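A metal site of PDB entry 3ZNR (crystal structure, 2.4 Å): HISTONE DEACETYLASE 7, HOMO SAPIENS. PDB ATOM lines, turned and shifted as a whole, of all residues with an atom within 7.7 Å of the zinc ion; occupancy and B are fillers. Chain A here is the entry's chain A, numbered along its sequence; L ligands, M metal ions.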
ATOM      1  N   PRO A 187     -26.808   5.692   9.367  1.00  0.00           N
ATOM      2  CA  PRO A 187     -27.546   6.844   8.830  1.00  0.00           C
ATOM      3  C   PRO A 187     -28.310   6.499   7.550  1.00  0.00           C
ATOM      4  O   PRO A 187     -28.192   5.386   7.044  1.00  0.00           O
ATOM      5  CB  PRO A 187     -26.433   7.860   8.529  1.00  0.00           C
ATOM      6  CG  PRO A 187     -25.217   7.025   8.314  1.00  0.00           C
ATOM      7  CD  PRO A 187     -25.346   5.870   9.243  1.00  0.00           C
ATOM      8  N   HIS A 189     -29.744   9.444   5.028  1.00  0.00           N
ATOM      9  CA  HIS A 189     -30.049  10.511   4.056  1.00  0.00           C
ATOM     10  C   HIS A 189     -29.234  10.515   2.756  1.00  0.00           C
ATOM     11  O   HIS A 189     -29.554  11.285   1.839  1.00  0.00           O
ATOM     12  CB  HIS A 189     -30.008  11.895   4.743  1.00  0.00           C
ATOM     13  CG  HIS A 189     -28.625  12.401   5.018  1.00  0.00           C
ATOM     14  ND1 HIS A 189     -28.315  13.746   4.951  1.00  0.00           N
ATOM     15  CD2 HIS A 189     -27.492  11.768   5.365  1.00  0.00           C
ATOM     16  CE1 HIS A 189     -27.039  13.905   5.242  1.00  0.00           C
ATOM     17  NE2 HIS A 189     -26.517  12.722   5.500  1.00  0.00           N
ATOM     18  N   HIS A 190     -28.199   9.687   2.653  1.00  0.00           N
ATOM     19  CA  HIS A 190     -27.473   9.502   1.397  1.00  0.00           C
ATOM     20  C   HIS A 190     -28.036   8.368   0.540  1.00  0.00           C
ATOM     21  O   HIS A 190     -27.837   8.346  -0.673  1.00  0.00           O
ATOM     22  CB  HIS A 190     -25.978   9.247   1.653  1.00  0.00           C
ATOM     23  CG  HIS A 190     -25.242  10.417   2.222  1.00  0.00           C
ATOM     24  ND1 HIS A 190     -25.352  11.687   1.705  1.00  0.00           N
ATOM     25  CD2 HIS A 190     -24.366  10.509   3.249  1.00  0.00           C
ATOM     26  CE1 HIS A 190     -24.584  12.510   2.393  1.00  0.00           C
ATOM     27  NE2 HIS A 190     -23.973  11.821   3.339  1.00  0.00           N
ATOM     28  N   GLY A 198     -22.349   6.324   1.123  1.00  0.00           N
ATOM     29  CA  GLY A 198     -22.026   7.228   2.227  1.00  0.00           C
ATOM     30  C   GLY A 198     -22.532   6.738   3.570  1.00  0.00           C
ATOM     31  O   GLY A 198     -23.232   7.458   4.276  1.00  0.00           O
ATOM     32  N   PHE A 199     -22.176   5.491   3.912  1.00  0.00           N
ATOM     33  CA  PHE A 199     -22.582   4.857   5.174  1.00  0.00           C
ATOM     34  C   PHE A 199     -24.093   4.629   5.315  1.00  0.00           C
ATOM     35  O   PHE A 199     -24.559   4.272   6.397  1.00  0.00           O
ATOM     36  CB  PHE A 199     -22.070   5.663   6.383  1.00  0.00           C
ATOM     37  CG  PHE A 199     -20.587   5.936   6.371  1.00  0.00           C
ATOM     38  CD1 PHE A 199     -19.691   5.010   6.888  1.00  0.00           C
ATOM     39  CD2 PHE A 199     -20.087   7.121   5.842  1.00  0.00           C
ATOM     40  CE1 PHE A 199     -18.325   5.252   6.878  1.00  0.00           C
ATOM     41  CE2 PHE A 199     -18.714   7.378   5.830  1.00  0.00           C
ATOM     42  CZ  PHE A 199     -17.841   6.439   6.354  1.00  0.00           C
ATOM     43  N   ASP A 225     -32.649  19.180   7.223  1.00  0.00           N
ATOM     44  CA  ASP A 225     -31.458  18.349   7.241  1.00  0.00           C
ATOM     45  C   ASP A 225     -30.238  19.261   7.469  1.00  0.00           C
ATOM     46  O   ASP A 225     -29.737  19.880   6.528  1.00  0.00           O
ATOM     47  CB  ASP A 225     -31.379  17.582   5.914  1.00  0.00           C
ATOM     48  CG  ASP A 225     -30.263  16.542   5.871  1.00  0.00           C
ATOM     49  OD1 ASP A 225     -29.289  16.660   6.652  1.00  0.00           O
ATOM     50  OD2 ASP A 225     -30.352  15.611   5.047  1.00  0.00           O
ATOM     51  N   TRP A 226     -29.788  19.344   8.716  1.00  0.00           N
ATOM     52  CA  TRP A 226     -28.655  20.221   9.065  1.00  0.00           C
ATOM     53  C   TRP A 226     -27.321  19.473   9.216  1.00  0.00           C
ATOM     54  O   TRP A 226     -26.340  20.040   9.699  1.00  0.00           O
ATOM     55  CB  TRP A 226     -28.972  21.057  10.323  1.00  0.00           C
ATOM     56  CG  TRP A 226     -29.215  20.295  11.596  1.00  0.00           C
ATOM     57  CD1 TRP A 226     -28.470  19.275  12.101  1.00  0.00           C
ATOM     58  CD2 TRP A 226     -30.266  20.529  12.537  1.00  0.00           C
ATOM     59  NE1 TRP A 226     -29.001  18.852  13.292  1.00  0.00           N
ATOM     60  CE2 TRP A 226     -30.098  19.609  13.585  1.00  0.00           C
ATOM     61  CE3 TRP A 226     -31.338  21.431  12.601  1.00  0.00           C
ATOM     62  CZ2 TRP A 226     -30.958  19.548  14.680  1.00  0.00           C
ATOM     63  CZ3 TRP A 226     -32.191  21.385  13.693  1.00  0.00           C
ATOM     64  CH2 TRP A 226     -31.997  20.448  14.714  1.00  0.00           C
ATOM     65  N   ASP A 227     -27.296  18.209   8.810  1.00  0.00           N
ATOM     66  CA  ASP A 227     -26.045  17.471   8.645  1.00  0.00           C
ATOM     67  C   ASP A 227     -25.198  18.218   7.613  1.00  0.00           C
ATOM     68  O   ASP A 227     -25.754  18.779   6.661  1.00  0.00           O
ATOM     69  CB  ASP A 227     -26.361  16.046   8.170  1.00  0.00           C
ATOM     70  CG  ASP A 227     -25.133  15.179   8.020  1.00  0.00           C
ATOM     71  OD1 ASP A 227     -24.282  15.494   7.157  1.00  0.00           O
ATOM     72  OD2 ASP A 227     -25.020  14.172   8.744  1.00  0.00           O
ATOM     73  N   VAL A 228     -23.883  18.248   7.785  1.00  0.00           N
ATOM     74  CA  VAL A 228     -23.019  19.051   6.920  1.00  0.00           C
ATOM     75  C   VAL A 228     -23.004  18.589   5.457  1.00  0.00           C
ATOM     76  O   VAL A 228     -22.707  19.378   4.555  1.00  0.00           O
ATOM     77  CB  VAL A 228     -21.570  19.128   7.465  1.00  0.00           C
ATOM     78  CG1 VAL A 228     -20.813  17.826   7.182  1.00  0.00           C
ATOM     79  CG2 VAL A 228     -20.829  20.313   6.868  1.00  0.00           C
ATOM     80  N   HIS A 229     -23.342  17.319   5.211  1.00  0.00           N
ATOM     81  CA  HIS A 229     -23.406  16.772   3.854  1.00  0.00           C
ATOM     82  C   HIS A 229     -24.811  16.869   3.286  1.00  0.00           C
ATOM     83  O   HIS A 229     -25.783  16.885   4.039  1.00  0.00           O
ATOM     84  CB  HIS A 229     -22.962  15.311   3.853  1.00  0.00           C
ATOM     85  CG  HIS A 229     -21.610  15.090   4.459  1.00  0.00           C
ATOM     86  ND1 HIS A 229     -21.415  14.897   5.813  1.00  0.00           N
ATOM     87  CD2 HIS A 229     -20.380  15.044   3.890  1.00  0.00           C
ATOM     88  CE1 HIS A 229     -20.129  14.745   6.050  1.00  0.00           C
ATOM     89  NE2 HIS A 229     -19.477  14.820   4.904  1.00  0.00           N
ATOM     90  N   HIS A 230     -24.927  16.943   1.964  1.00  0.00           N
ATOM     91  CA  HIS A 230     -26.234  17.032   1.312  1.00  0.00           C
ATOM     92  C   HIS A 230     -26.952  15.683   1.330  1.00  0.00           C
ATOM     93  O   HIS A 230     -26.376  14.663   0.985  1.00  0.00           O
ATOM     94  CB  HIS A 230     -26.093  17.521  -0.128  1.00  0.00           C
ATOM     95  CG  HIS A 230     -27.394  17.630  -0.863  1.00  0.00           C
ATOM     96  ND1 HIS A 230     -27.695  16.853  -1.959  1.00  0.00           N
ATOM     97  CD2 HIS A 230     -28.483  18.409  -0.640  1.00  0.00           C
ATOM     98  CE1 HIS A 230     -28.909  17.161  -2.387  1.00  0.00           C
ATOM     99  NE2 HIS A 230     -29.405  18.103  -1.611  1.00  0.00           N
ATOM    100  N   PHE A 257     -17.428  18.626  -2.643  1.00  0.00           N
ATOM    101  CA  PHE A 257     -17.615  18.096  -1.298  1.00  0.00           C
ATOM    102  C   PHE A 257     -18.747  17.059  -1.328  1.00  0.00           C
ATOM    103  O   PHE A 257     -19.742  17.265  -2.010  1.00  0.00           O
ATOM    104  CB  PHE A 257     -17.949  19.217  -0.312  1.00  0.00           C
ATOM    105  CG  PHE A 257     -17.883  18.797   1.135  1.00  0.00           C
ATOM    106  CD1 PHE A 257     -16.659  18.674   1.781  1.00  0.00           C
ATOM    107  CD2 PHE A 257     -19.049  18.547   1.855  1.00  0.00           C
ATOM    108  CE1 PHE A 257     -16.587  18.288   3.115  1.00  0.00           C
ATOM    109  CE2 PHE A 257     -18.982  18.170   3.189  1.00  0.00           C
ATOM    110  CZ  PHE A 257     -17.757  18.037   3.821  1.00  0.00           C
ATOM    111  N   PHE A 258     -18.582  15.965  -0.596  1.00  0.00           N
ATOM    112  CA  PHE A 258     -19.506  14.830  -0.687  1.00  0.00           C
ATOM    113  C   PHE A 258     -20.929  15.237  -0.264  1.00  0.00           C
ATOM    114  O   PHE A 258     -21.095  15.971   0.706  1.00  0.00           O
ATOM    115  CB  PHE A 258     -19.029  13.659   0.182  1.00  0.00           C
ATOM    116  CG  PHE A 258     -19.796  12.380  -0.056  1.00  0.00           C
ATOM    117  CD1 PHE A 258     -20.991  12.140   0.619  1.00  0.00           C
ATOM    118  CD2 PHE A 258     -19.333  11.440  -0.963  1.00  0.00           C
ATOM    119  CE1 PHE A 258     -21.706  10.969   0.397  1.00  0.00           C
ATOM    120  CE2 PHE A 258     -20.043  10.260  -1.186  1.00  0.00           C
ATOM    121  CZ  PHE A 258     -21.230  10.025  -0.506  1.00  0.00           C
ATOM    122  N   GLY A 319     -27.789  15.396  11.708  1.00  0.00           N
ATOM    123  CA  GLY A 319     -26.368  15.105  11.730  1.00  0.00           C
ATOM    124  C   GLY A 319     -25.646  16.184  12.506  1.00  0.00           C
ATOM    125  O   GLY A 319     -26.060  17.341  12.500  1.00  0.00           O
ATOM    126  N   PHE A 320     -24.566  15.806  13.193  1.00  0.00           N
ATOM    127  CA  PHE A 320     -23.784  16.757  13.978  1.00  0.00           C
ATOM    128  C   PHE A 320     -22.330  16.828  13.512  1.00  0.00           C
ATOM    129  O   PHE A 320     -21.430  17.087  14.316  1.00  0.00           O
ATOM    130  CB  PHE A 320     -23.863  16.392  15.466  1.00  0.00           C
ATOM    131  CG  PHE A 320     -25.267  16.367  15.996  1.00  0.00           C
ATOM    132  CD1 PHE A 320     -25.984  17.552  16.131  1.00  0.00           C
ATOM    133  CD2 PHE A 320     -25.890  15.162  16.331  1.00  0.00           C
ATOM    134  CE1 PHE A 320     -27.292  17.539  16.607  1.00  0.00           C
ATOM    135  CE2 PHE A 320     -27.190  15.153  16.811  1.00  0.00           C
ATOM    136  CZ  PHE A 320     -27.895  16.345  16.943  1.00  0.00           C
ATOM    137  N   ASP A 321     -22.118  16.636  12.212  1.00  0.00           N
ATOM    138  CA  ASP A 321     -20.778  16.710  11.622  1.00  0.00           C
ATOM    139  C   ASP A 321     -20.417  18.123  11.149  1.00  0.00           C
ATOM    140  O   ASP A 321     -19.328  18.340  10.613  1.00  0.00           O
ATOM    141  CB  ASP A 321     -20.606  15.681  10.496  1.00  0.00           C
ATOM    142  CG  ASP A 321     -21.791  15.631   9.530  1.00  0.00           C
ATOM    143  OD1 ASP A 321     -22.666  16.527   9.595  1.00  0.00           O
ATOM    144  OD2 ASP A 321     -21.844  14.697   8.711  1.00  0.00           O
ATOM    145  N   ALA A 322     -21.325  19.072  11.343  1.00  0.00           N
ATOM    146  CA  ALA A 322     -21.026  20.498  11.171  1.00  0.00           C
ATOM    147  C   ALA A 322     -20.523  21.109  12.483  1.00  0.00           C
ATOM    148  O   ALA A 322     -20.179  22.293  12.529  1.00  0.00           O
ATOM    149  CB  ALA A 322     -22.254  21.250  10.678  1.00  0.00           C
ATOM    150  N   LEU A 330     -14.039  16.150   6.523  1.00  0.00           N
ATOM    151  CA  LEU A 330     -15.238  15.581   7.142  1.00  0.00           C
ATOM    152  C   LEU A 330     -16.301  16.662   7.330  1.00  0.00           C
ATOM    153  O   LEU A 330     -17.480  16.416   7.080  1.00  0.00           O
ATOM    154  CB  LEU A 330     -14.899  14.929   8.493  1.00  0.00           C
ATOM    155  CG  LEU A 330     -16.074  14.425   9.343  1.00  0.00           C
ATOM    156  CD1 LEU A 330     -17.071  13.609   8.523  1.00  0.00           C
ATOM    157  CD2 LEU A 330     -15.551  13.612  10.519  1.00  0.00           C
ATOM    158  N   GLU A 360     -28.065  11.333  12.101  1.00  0.00           N
ATOM    159  CA  GLU A 360     -27.451  11.031  10.809  1.00  0.00           C
ATOM    160  C   GLU A 360     -25.934  10.941  11.004  1.00  0.00           C
ATOM    161  O   GLU A 360     -25.442   9.920  11.478  1.00  0.00           O
ATOM    162  CB  GLU A 360     -27.842  12.078   9.765  1.00  0.00           C
ATOM    163  CG  GLU A 360     -29.343  12.171   9.485  1.00  0.00           C
ATOM    164  CD  GLU A 360     -29.871  11.073   8.565  1.00  0.00           C
ATOM    165  OE1 GLU A 360     -29.113  10.129   8.241  1.00  0.00           O
ATOM    166  OE2 GLU A 360     -31.048  11.158   8.173  1.00  0.00           O
ATOM    167  N   GLY A 361     -25.194  12.004  10.679  1.00  0.00           N
ATOM    168  CA  GLY A 361     -23.739  12.013  10.773  1.00  0.00           C
ATOM    169  C   GLY A 361     -23.215  12.577  12.091  1.00  0.00           C
ATOM    170  O   GLY A 361     -23.996  12.895  12.993  1.00  0.00           O
ATOM    171  N   GLY A 362     -21.892  12.697  12.182  1.00  0.00           N
ATOM    172  CA  GLY A 362     -21.208  13.153  13.379  1.00  0.00           C
ATOM    173  C   GLY A 362     -20.283  12.070  13.915  1.00  0.00           C
ATOM    174  O   GLY A 362     -20.733  10.975  14.219  1.00  0.00           O
HETATM  175  F1  LIG L   1     -24.095  10.021   8.447  1.00  0.00           F
HETATM  176  C1  LIG L   1     -24.098  10.650   7.276  1.00  0.00           C
HETATM  177  F2  LIG L   1     -24.699   9.889   6.365  1.00  0.00           F
HETATM  178  F3  LIG L   1     -24.739  11.811   7.393  1.00  0.00           F
HETATM  179  C2  LIG L   1     -22.696  10.929   6.866  1.00  0.00           C
HETATM  180  N1  LIG L   1     -22.143  10.585   5.681  1.00  0.00           N
HETATM  181  C3  LIG L   1     -20.825  11.065   5.660  1.00  0.00           C
HETATM  182  N2  LIG L   1     -20.586  11.652   6.859  1.00  0.00           N
HETATM  183  O1  LIG L   1     -21.750  11.607   7.614  1.00  0.00           O
HETATM  184  C4  LIG L   1     -19.900  10.847   4.640  1.00  0.00           C
HETATM  185  C5  LIG L   1     -20.291  10.198   3.463  1.00  0.00           C
HETATM  186  C6  LIG L   1     -19.361   9.972   2.443  1.00  0.00           C
HETATM  187  C7  LIG L   1     -18.036  10.397   2.592  1.00  0.00           C
HETATM  188  C8  LIG L   1     -17.642  11.049   3.761  1.00  0.00           C
HETATM  189  C9  LIG L   1     -18.571  11.264   4.789  1.00  0.00           C
HETATM  190  C10 LIG L   1     -16.233  11.484   3.954  1.00  0.00           C
HETATM  191  O2  LIG L   1     -15.665  12.221   3.155  1.00  0.00           O
HETATM  192  N3  LIG L   1     -15.592  10.978   5.128  1.00  0.00           N
HETATM  193  C11 LIG L   1     -14.236  11.269   5.491  1.00  0.00           C
HETATM  194  C12 LIG L   1     -13.484  10.174   6.299  1.00  0.00           C
HETATM  195  C13 LIG L   1     -12.076  10.709   6.375  1.00  0.00           C
HETATM  196  C14 LIG L   1     -11.054   9.602   6.705  1.00  0.00           C
HETATM  197  O3  LIG L   1     -11.627   8.294   6.785  1.00  0.00           O
HETATM  198  C15 LIG L   1     -12.475   7.948   5.674  1.00  0.00           C
HETATM  199  C16 LIG L   1     -13.590   8.975   5.410  1.00  0.00           C
HETATM  200  C17 LIG L   1     -14.287  10.133   7.569  1.00  0.00           C
HETATM  201  N4  LIG L   1     -15.706   9.706   7.664  1.00  0.00           N
HETATM  202  C18 LIG L   1     -16.235   9.855   9.201  1.00  0.00           C
HETATM  203  C19 LIG L   1     -15.121  10.303   9.988  1.00  0.00           C
HETATM  204  S1  LIG L   1     -13.846  10.494   9.011  1.00  0.00           S
HETATM  205  C20 LIG L   1     -17.531   9.567   9.613  1.00  0.00           C
HETATM  206  C21 LIG L   1     -18.570   9.584   8.671  1.00  0.00           C
HETATM  207  C22 LIG L   1     -19.887   9.308   9.065  1.00  0.00           C
HETATM  208  C23 LIG L   1     -20.170   9.000  10.404  1.00  0.00           C
HETATM  209  C24 LIG L   1     -19.135   8.992  11.347  1.00  0.00           C
HETATM  210  C25 LIG L   1     -17.819   9.268  10.952  1.00  0.00           C
HETATM  211 ZN    ZN M   1     -22.785  14.031   7.178  1.00  0.00          ZN
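The side-chain carboxylate of Asp 225 lies within hydrogen-bond range of the backbone NH of Asp 227 (3.3 Å).
The backbone NH (N) of Val 228 lies within hydrogen-bond range of the side-chain carboxylate (OD1) of Asp 321, at 2.8 Å.
The side-chain carboxylate (OD2) of Asp 227 lies within hydrogen-bond range of the backbone NH (N) of Gly 361 (2.9 Å).
NE2 of His 229 sits close to O of Leu 330 (3.4 Å).
A nitrogen (N1) of the ligand sits at hydrogen-bond distance from a ring nitrogen (NE2) of His 190.
Three residues have an atom within 4 Å of the zinc ion: Asp 227, His 229 and Asp 321.
The nearest printed residue that does not touch the zinc ion is Gly 361 (4.2 Å).
The side-chain carboxylate (OD2) of Asp 321 is bound to the zinc ion (1.9 Å).
OD1 of Asp 227 is bound to the zinc ion (2.1 Å).
The zinc ion is bound by a ring nitrogen (ND1) of His 229 (2.1 Å).
The zinc ion has three donor atoms within binding distance.
Slightly farther from the zinc ion lies O1 of the ligand (2.7 Å).
Slightly farther from the zinc ion lies OD2 of Asp 227 (2.7 Å).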
